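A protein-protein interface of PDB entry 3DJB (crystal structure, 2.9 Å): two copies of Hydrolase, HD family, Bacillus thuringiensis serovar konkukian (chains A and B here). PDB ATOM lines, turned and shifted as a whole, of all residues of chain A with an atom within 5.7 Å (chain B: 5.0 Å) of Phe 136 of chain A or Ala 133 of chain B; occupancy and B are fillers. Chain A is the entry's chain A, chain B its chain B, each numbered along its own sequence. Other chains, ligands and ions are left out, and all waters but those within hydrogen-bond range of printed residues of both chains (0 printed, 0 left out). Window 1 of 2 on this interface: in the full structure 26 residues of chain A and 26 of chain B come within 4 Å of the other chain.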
ATOM      1  N   GLY A 131      30.307  23.162 -12.258  1.00  0.00           N
ATOM      2  CA  GLY A 131      31.203  22.402 -11.408  1.00  0.00           C
ATOM      3  C   GLY A 131      30.372  21.545 -10.488  1.00  0.00           C
ATOM      4  O   GLY A 131      30.485  20.322 -10.493  1.00  0.00           O
ATOM      5  N   ILE A 132      29.537  22.199  -9.690  1.00  0.00           N
ATOM      6  CA  ILE A 132      28.649  21.502  -8.785  1.00  0.00           C
ATOM      7  C   ILE A 132      28.097  20.304  -9.542  1.00  0.00           C
ATOM      8  O   ILE A 132      28.291  19.163  -9.134  1.00  0.00           O
ATOM      9  CB  ILE A 132      27.496  22.442  -8.355  1.00  0.00           C
ATOM     10  CG1 ILE A 132      28.072  23.597  -7.498  1.00  0.00           C
ATOM     11  CG2 ILE A 132      26.427  21.651  -7.619  1.00  0.00           C
ATOM     12  CD1 ILE A 132      27.233  24.905  -7.426  1.00  0.00           C
ATOM     13  N   ALA A 133      27.445  20.560 -10.668  1.00  0.00           N
ATOM     14  CA  ALA A 133      26.883  19.467 -11.445  1.00  0.00           C
ATOM     15  C   ALA A 133      27.953  18.500 -11.856  1.00  0.00           C
ATOM     16  O   ALA A 133      27.869  17.321 -11.549  1.00  0.00           O
ATOM     17  CB  ALA A 133      26.163  19.983 -12.677  1.00  0.00           C
ATOM     18  N   ARG A 134      28.977  18.974 -12.543  1.00  0.00           N
ATOM     19  CA  ARG A 134      29.997  18.034 -12.967  1.00  0.00           C
ATOM     20  C   ARG A 134      30.349  17.090 -11.835  1.00  0.00           C
ATOM     21  O   ARG A 134      30.545  15.901 -12.049  1.00  0.00           O
ATOM     22  CB  ARG A 134      31.247  18.756 -13.423  1.00  0.00           C
ATOM     23  CG  ARG A 134      32.201  17.868 -14.173  1.00  0.00           C
ATOM     24  CD  ARG A 134      33.281  18.747 -14.756  1.00  0.00           C
ATOM     25  NE  ARG A 134      32.675  19.804 -15.570  1.00  0.00           N
ATOM     26  CZ  ARG A 134      32.968  21.103 -15.481  1.00  0.00           C
ATOM     27  NH1 ARG A 134      33.872  21.543 -14.609  1.00  0.00           N
ATOM     28  NH2 ARG A 134      32.353  21.969 -16.274  1.00  0.00           N
ATOM     29  N   THR A 135      30.378  17.622 -10.621  1.00  0.00           N
ATOM     30  CA  THR A 135      30.732  16.822  -9.459  1.00  0.00           C
ATOM     31  C   THR A 135      29.736  15.707  -9.120  1.00  0.00           C
ATOM     32  O   THR A 135      30.045  14.527  -9.289  1.00  0.00           O
ATOM     33  CB  THR A 135      30.967  17.714  -8.219  1.00  0.00           C
ATOM     34  OG1 THR A 135      31.507  18.976  -8.632  1.00  0.00           O
ATOM     35  CG2 THR A 135      31.986  17.057  -7.301  1.00  0.00           C
ATOM     36  N   PHE A 136      28.557  16.056  -8.633  1.00  0.00           N
ATOM     37  CA  PHE A 136      27.582  15.028  -8.306  1.00  0.00           C
ATOM     38  C   PHE A 136      27.412  14.056  -9.459  1.00  0.00           C
ATOM     39  O   PHE A 136      27.170  12.858  -9.249  1.00  0.00           O
ATOM     40  CB  PHE A 136      26.272  15.686  -7.964  1.00  0.00           C
ATOM     41  CG  PHE A 136      26.372  16.581  -6.790  1.00  0.00           C
ATOM     42  CD1 PHE A 136      26.625  16.052  -5.539  1.00  0.00           C
ATOM     43  CD2 PHE A 136      26.212  17.947  -6.920  1.00  0.00           C
ATOM     44  CE1 PHE A 136      26.700  16.865  -4.431  1.00  0.00           C
ATOM     45  CE2 PHE A 136      26.287  18.768  -5.809  1.00  0.00           C
ATOM     46  CZ  PHE A 136      26.531  18.228  -4.568  1.00  0.00           C
ATOM     47  N   ALA A 137      27.559  14.575 -10.677  1.00  0.00           N
ATOM     48  CA  ALA A 137      27.443  13.782 -11.904  1.00  0.00           C
ATOM     49  C   ALA A 137      28.525  12.719 -11.919  1.00  0.00           C
ATOM     50  O   ALA A 137      28.244  11.530 -12.022  1.00  0.00           O
ATOM     51  CB  ALA A 137      27.604  14.683 -13.111  1.00  0.00           C
ATOM     52  N   TYR A 138      29.771  13.172 -11.833  1.00  0.00           N
ATOM     53  CA  TYR A 138      30.904  12.274 -11.804  1.00  0.00           C
ATOM     54  C   TYR A 138      30.736  11.335 -10.599  1.00  0.00           C
ATOM     55  O   TYR A 138      31.142  10.161 -10.631  1.00  0.00           O
ATOM     56  CB  TYR A 138      32.183  13.090 -11.683  1.00  0.00           C
ATOM     57  CG  TYR A 138      33.391  12.278 -11.306  1.00  0.00           C
ATOM     58  CD1 TYR A 138      33.843  11.242 -12.131  1.00  0.00           C
ATOM     59  CD2 TYR A 138      34.087  12.543 -10.120  1.00  0.00           C
ATOM     60  CE1 TYR A 138      34.958  10.482 -11.788  1.00  0.00           C
ATOM     61  CE2 TYR A 138      35.200  11.793  -9.765  1.00  0.00           C
ATOM     62  CZ  TYR A 138      35.634  10.760 -10.609  1.00  0.00           C
ATOM     63  OH  TYR A 138      36.740  10.013 -10.272  1.00  0.00           O
ATOM     64  N   GLY A 139      30.122  11.863  -9.540  1.00  0.00           N
ATOM     65  CA  GLY A 139      29.880  11.078  -8.343  1.00  0.00           C
ATOM     66  C   GLY A 139      28.923   9.942  -8.640  1.00  0.00           C
ATOM     67  O   GLY A 139      29.161   8.797  -8.255  1.00  0.00           O
ATOM     68  N   GLY A 140      27.834  10.259  -9.329  1.00  0.00           N
ATOM     69  CA  GLY A 140      26.875   9.232  -9.686  1.00  0.00           C
ATOM     70  C   GLY A 140      27.513   8.103 -10.474  1.00  0.00           C
ATOM     71  O   GLY A 140      27.327   6.929 -10.152  1.00  0.00           O
ATOM     72  N   ALA A 141      28.266   8.463 -11.512  1.00  0.00           N
ATOM     73  CA  ALA A 141      28.950   7.487 -12.350  1.00  0.00           C
ATOM     74  C   ALA A 141      29.918   6.680 -11.500  1.00  0.00           C
ATOM     75  O   ALA A 141      29.853   5.456 -11.469  1.00  0.00           O
ATOM     76  CB  ALA A 141      29.701   8.187 -13.464  1.00  0.00           C
ATOM     77  N   MET A 146      26.377  11.648  -2.015  1.00  0.00           N
ATOM     78  CA  MET A 146      26.551  13.066  -2.289  1.00  0.00           C
ATOM     79  C   MET A 146      27.205  13.725  -1.085  1.00  0.00           C
ATOM     80  O   MET A 146      28.105  14.554  -1.224  1.00  0.00           O
ATOM     81  CB  MET A 146      25.206  13.716  -2.545  1.00  0.00           C
ATOM     82  CG  MET A 146      24.190  12.768  -3.083  1.00  0.00           C
ATOM     83  SD  MET A 146      22.652  13.722  -3.721  1.00  0.00           S
ATOM     84  CE  MET A 146      22.283  14.884  -2.223  1.00  0.00           C
ATOM     85  N   SER A 169      30.680  13.057  -2.916  1.00  0.00           N
ATOM     86  CA  SER A 169      30.802  14.129  -3.895  1.00  0.00           C
ATOM     87  C   SER A 169      30.905  15.519  -3.311  1.00  0.00           C
ATOM     88  O   SER A 169      31.618  16.354  -3.844  1.00  0.00           O
ATOM     89  CB  SER A 169      29.618  14.107  -4.860  1.00  0.00           C
ATOM     90  OG  SER A 169      29.487  12.844  -5.488  1.00  0.00           O
ATOM     91  N   LEU A 170      30.191  15.783  -2.229  1.00  0.00           N
ATOM     92  CA  LEU A 170      30.228  17.114  -1.642  1.00  0.00           C
ATOM     93  C   LEU A 170      31.600  17.476  -1.118  1.00  0.00           C
ATOM     94  O   LEU A 170      32.002  18.639  -1.168  1.00  0.00           O
ATOM     95  CB  LEU A 170      29.227  17.248  -0.500  1.00  0.00           C
ATOM     96  CG  LEU A 170      29.077  18.685  -0.012  1.00  0.00           C
ATOM     97  CD1 LEU A 170      27.900  19.302  -0.694  1.00  0.00           C
ATOM     98  CD2 LEU A 170      28.876  18.708   1.478  1.00  0.00           C
ATOM     99  N   PHE A 173      34.416  19.289  -3.167  1.00  0.00           N
ATOM    100  CA  PHE A 173      34.443  20.736  -3.266  1.00  0.00           C
ATOM    101  C   PHE A 173      35.594  21.316  -2.462  1.00  0.00           C
ATOM    102  O   PHE A 173      36.504  21.936  -3.025  1.00  0.00           O
ATOM    103  CB  PHE A 173      33.103  21.319  -2.823  1.00  0.00           C
ATOM    104  CG  PHE A 173      31.972  20.989  -3.761  1.00  0.00           C
ATOM    105  CD1 PHE A 173      30.913  20.200  -3.342  1.00  0.00           C
ATOM    106  CD2 PHE A 173      32.005  21.414  -5.090  1.00  0.00           C
ATOM    107  CE1 PHE A 173      29.912  19.845  -4.225  1.00  0.00           C
ATOM    108  CE2 PHE A 173      31.002  21.059  -5.977  1.00  0.00           C
ATOM    109  CZ  PHE A 173      29.961  20.271  -5.545  1.00  0.00           C
ATOM    110  N   PHE A 203      25.933  27.779  -2.267  1.00  0.00           N
ATOM    111  CA  PHE A 203      25.249  26.534  -2.612  1.00  0.00           C
ATOM    112  C   PHE A 203      25.389  25.526  -1.465  1.00  0.00           C
ATOM    113  O   PHE A 203      24.386  25.082  -0.899  1.00  0.00           O
ATOM    114  CB  PHE A 203      25.830  25.943  -3.900  1.00  0.00           C
ATOM    115  CG  PHE A 203      25.318  24.570  -4.220  1.00  0.00           C
ATOM    116  CD1 PHE A 203      25.898  23.445  -3.650  1.00  0.00           C
ATOM    117  CD2 PHE A 203      24.255  24.401  -5.087  1.00  0.00           C
ATOM    118  CE1 PHE A 203      25.420  22.167  -3.940  1.00  0.00           C
ATOM    119  CE2 PHE A 203      23.773  23.128  -5.380  1.00  0.00           C
ATOM    120  CZ  PHE A 203      24.358  22.011  -4.806  1.00  0.00           C
ATOM    121  N   PHE A 207      22.662  23.833   0.573  1.00  0.00           N
ATOM    122  CA  PHE A 207      22.592  22.386   0.549  1.00  0.00           C
ATOM    123  C   PHE A 207      22.555  21.834   1.948  1.00  0.00           C
ATOM    124  O   PHE A 207      21.777  20.938   2.235  1.00  0.00           O
ATOM    125  CB  PHE A 207      23.794  21.808  -0.195  1.00  0.00           C
ATOM    126  CG  PHE A 207      23.885  20.299  -0.162  1.00  0.00           C
ATOM    127  CD1 PHE A 207      24.346  19.631   0.966  1.00  0.00           C
ATOM    128  CD2 PHE A 207      23.571  19.551  -1.292  1.00  0.00           C
ATOM    129  CE1 PHE A 207      24.497  18.242   0.956  1.00  0.00           C
ATOM    130  CE2 PHE A 207      23.720  18.166  -1.303  1.00  0.00           C
ATOM    131  CZ  PHE A 207      24.185  17.515  -0.183  1.00  0.00           C
ATOM    132  N   ALA B 129      18.875  22.590  -3.456  1.00  0.00           N
ATOM    133  CA  ALA B 129      20.231  22.125  -3.704  1.00  0.00           C
ATOM    134  C   ALA B 129      20.293  20.600  -3.867  1.00  0.00           C
ATOM    135  O   ALA B 129      20.726  20.098  -4.912  1.00  0.00           O
ATOM    136  CB  ALA B 129      21.137  22.572  -2.567  1.00  0.00           C
ATOM    137  N   ILE B 130      19.850  19.877  -2.833  1.00  0.00           N
ATOM    138  CA  ILE B 130      19.838  18.404  -2.809  1.00  0.00           C
ATOM    139  C   ILE B 130      19.256  17.835  -4.123  1.00  0.00           C
ATOM    140  O   ILE B 130      19.802  16.892  -4.719  1.00  0.00           O
ATOM    141  CB  ILE B 130      18.972  17.857  -1.600  1.00  0.00           C
ATOM    142  CG1 ILE B 130      19.191  18.708  -0.340  1.00  0.00           C
ATOM    143  CG2 ILE B 130      19.338  16.396  -1.294  1.00  0.00           C
ATOM    144  CD1 ILE B 130      20.606  18.671   0.197  1.00  0.00           C
ATOM    145  N   GLY B 131      18.131  18.419  -4.549  1.00  0.00           N
ATOM    146  CA  GLY B 131      17.463  17.993  -5.765  1.00  0.00           C
ATOM    147  C   GLY B 131      18.431  18.131  -6.907  1.00  0.00           C
ATOM    148  O   GLY B 131      18.740  17.162  -7.582  1.00  0.00           O
ATOM    149  N   ILE B 132      18.909  19.350  -7.120  1.00  0.00           N
ATOM    150  CA  ILE B 132      19.879  19.620  -8.159  1.00  0.00           C
ATOM    151  C   ILE B 132      20.888  18.478  -8.118  1.00  0.00           C
ATOM    152  O   ILE B 132      21.057  17.754  -9.102  1.00  0.00           O
ATOM    153  CB  ILE B 132      20.586  20.964  -7.887  1.00  0.00           C
ATOM    154  CG1 ILE B 132      19.566  22.114  -8.034  1.00  0.00           C
ATOM    155  CG2 ILE B 132      21.772  21.122  -8.818  1.00  0.00           C
ATOM    156  CD1 ILE B 132      19.889  23.430  -7.286  1.00  0.00           C
ATOM    157  N   ALA B 133      21.530  18.288  -6.971  1.00  0.00           N
ATOM    158  CA  ALA B 133      22.510  17.220  -6.860  1.00  0.00           C
ATOM    159  C   ALA B 133      21.893  15.889  -7.153  1.00  0.00           C
ATOM    160  O   ALA B 133      22.354  15.178  -8.030  1.00  0.00           O
ATOM    161  CB  ALA B 133      23.132  17.197  -5.482  1.00  0.00           C
ATOM    162  N   ARG B 134      20.844  15.530  -6.436  1.00  0.00           N
ATOM    163  CA  ARG B 134      20.259  14.225  -6.705  1.00  0.00           C
ATOM    164  C   ARG B 134      20.132  13.997  -8.205  1.00  0.00           C
ATOM    165  O   ARG B 134      20.380  12.900  -8.694  1.00  0.00           O
ATOM    166  CB  ARG B 134      18.888  14.101  -6.063  1.00  0.00           C
ATOM    167  CG  ARG B 134      18.377  12.687  -6.027  1.00  0.00           C
ATOM    168  CD  ARG B 134      17.133  12.660  -5.181  1.00  0.00           C
ATOM    169  NE  ARG B 134      17.419  13.239  -3.867  1.00  0.00           N
ATOM    170  CZ  ARG B 134      16.693  14.184  -3.267  1.00  0.00           C
ATOM    171  NH1 ARG B 134      15.605  14.693  -3.845  1.00  0.00           N
ATOM    172  NH2 ARG B 134      17.062  14.628  -2.075  1.00  0.00           N
ATOM    173  N   THR B 135      19.793  15.054  -8.934  1.00  0.00           N
ATOM    174  CA  THR B 135      19.610  14.951 -10.375  1.00  0.00           C
ATOM    175  C   THR B 135      20.889  14.634 -11.156  1.00  0.00           C
ATOM    176  O   THR B 135      21.030  13.535 -11.694  1.00  0.00           O
ATOM    177  CB  THR B 135      18.947  16.228 -10.947  1.00  0.00           C
ATOM    178  OG1 THR B 135      18.048  16.785  -9.977  1.00  0.00           O
ATOM    179  CG2 THR B 135      18.126  15.875 -12.174  1.00  0.00           C
ATOM    180  N   PHE B 136      21.816  15.573 -11.240  1.00  0.00           N
ATOM    181  CA  PHE B 136      23.044  15.293 -11.966  1.00  0.00           C
ATOM    182  C   PHE B 136      23.659  13.970 -11.520  1.00  0.00           C
ATOM    183  O   PHE B 136      24.270  13.245 -12.326  1.00  0.00           O
ATOM    184  CB  PHE B 136      24.013  16.434 -11.758  1.00  0.00           C
ATOM    185  CG  PHE B 136      23.494  17.725 -12.261  1.00  0.00           C
ATOM    186  CD1 PHE B 136      23.312  17.914 -13.618  1.00  0.00           C
ATOM    187  CD2 PHE B 136      23.198  18.758 -11.394  1.00  0.00           C
ATOM    188  CE1 PHE B 136      22.842  19.112 -14.104  1.00  0.00           C
ATOM    189  CE2 PHE B 136      22.727  19.958 -11.877  1.00  0.00           C
ATOM    190  CZ  PHE B 136      22.555  20.137 -13.229  1.00  0.00           C
ATOM    191  N   ALA B 137      23.475  13.657 -10.237  1.00  0.00           N
ATOM    192  CA  ALA B 137      23.983  12.423  -9.638  1.00  0.00           C
ATOM    193  C   ALA B 137      23.342  11.232 -10.326  1.00  0.00           C
ATOM    194  O   ALA B 137      24.023  10.369 -10.874  1.00  0.00           O
ATOM    195  CB  ALA B 137      23.650  12.396  -8.161  1.00  0.00           C
ATOM    196  N   TYR B 138      22.017  11.195 -10.276  1.00  0.00           N
ATOM    197  CA  TYR B 138      21.266  10.135 -10.910  1.00  0.00           C
ATOM    198  C   TYR B 138      21.621  10.128 -12.403  1.00  0.00           C
ATOM    199  O   TYR B 138      21.642   9.072 -13.058  1.00  0.00           O
ATOM    200  CB  TYR B 138      19.778  10.394 -10.709  1.00  0.00           C
ATOM    201  CG  TYR B 138      18.887   9.562 -11.590  1.00  0.00           C
ATOM    202  CD1 TYR B 138      18.915   8.162 -11.519  1.00  0.00           C
ATOM    203  CD2 TYR B 138      18.019  10.171 -12.503  1.00  0.00           C
ATOM    204  CE1 TYR B 138      18.099   7.383 -12.333  1.00  0.00           C
ATOM    205  CE2 TYR B 138      17.201   9.407 -13.324  1.00  0.00           C
ATOM    206  CZ  TYR B 138      17.246   8.009 -13.233  1.00  0.00           C
ATOM    207  OH  TYR B 138      16.438   7.241 -14.040  1.00  0.00           O
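The side-chain sulfur (SD) of Met 146 of chain A sits at hydrogen-bond distance from the backbone NH (N) of Arg 134 of chain B (3.7 Å).
N of Leu 170 of chain A is in hydrogen-bond range of O of Met 146 of chain A (2.6 Å). The backbone carbonyl oxygen (O) of Met 146 of chain A lies within hydrogen-bond range of the backbone NH (N) of Ser 169 of chain A, at 3.4 Å.
Ala 133 of chain A touches Phe 136 of chain B. Ala 133 of chain B touches Phe 136 of chain A. Ala 137 of chain B touches Phe 136 of chain A (CA to O, 3.2 Å). Ala 137 of chain A touches Phe 136 of chain B. CA of Gly 140 of chain A touches O of Ala 137 of chain B, 3.3 Å away. Met 146 of chain A touches Ile 130 of chain B. Met 146 of chain A touches Ala 133 of chain B. Phe 203 of chain A touches Ala 129 of chain B (CE2 to CB, 3.9 Å). CB of Ala 129 of chain B touches CA of Phe 207 of chain A, at 3.4 Å. Ile 130 of chain B touches Phe 207 of chain A.
Phe 136 of chain A touches just these residues of chain B: Ala 133 and Ala 137. Of chain A, only Phe 136 and Met 146 come within 4 Å of Ala 133 of chain B. Printed residues of chain B within 4 Å of Phe 207 of chain A: Ala 129 and Ile 130. Of the printed residues of chain A, Ala 129 of chain B touches Phe 203 and Phe 207. Of the printed residues of chain B, Ala 137 of chain A touches Phe 136. Arg 134 of chain A touches none of the printed residues of chain B. The nearest residue of chain A that does not touch Ala 133 of chain B is Phe 207 of chain A (4.3 Å). The nearest printed residue of chain A that does not touch Arg 134 of chain B is Phe 136 of chain A (5.6 Å).
Hydrophobic or aromatic side chains of chain B within 4 Å of the printed part of chain A: Ala 129, Ile 130, Ala 133, Phe 136 and Ala 137. Printed residues of chain A that touch a printed residue of chain B: Ala 133, Phe 136, Ala 137, Gly 140, Met 146, Phe 203 and Phe 207. Hydrophobic or aromatic side chains of chain A that line the printed part of chain B: Ala 133, Phe 136, Ala 137, Met 146, Phe 203 and Phe 207. Among the printed residues, 11 pairs touch across the chains.
Ala 133 of chain A touches Phe 136 of chain B, and with the chains exchanged Phe 136 of chain A touches Ala 133 of chain B. Phe 136 of chain A touches Ala 137 of chain B, and with the chains exchanged Ala 137 of chain A touches Phe 136 of chain B.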
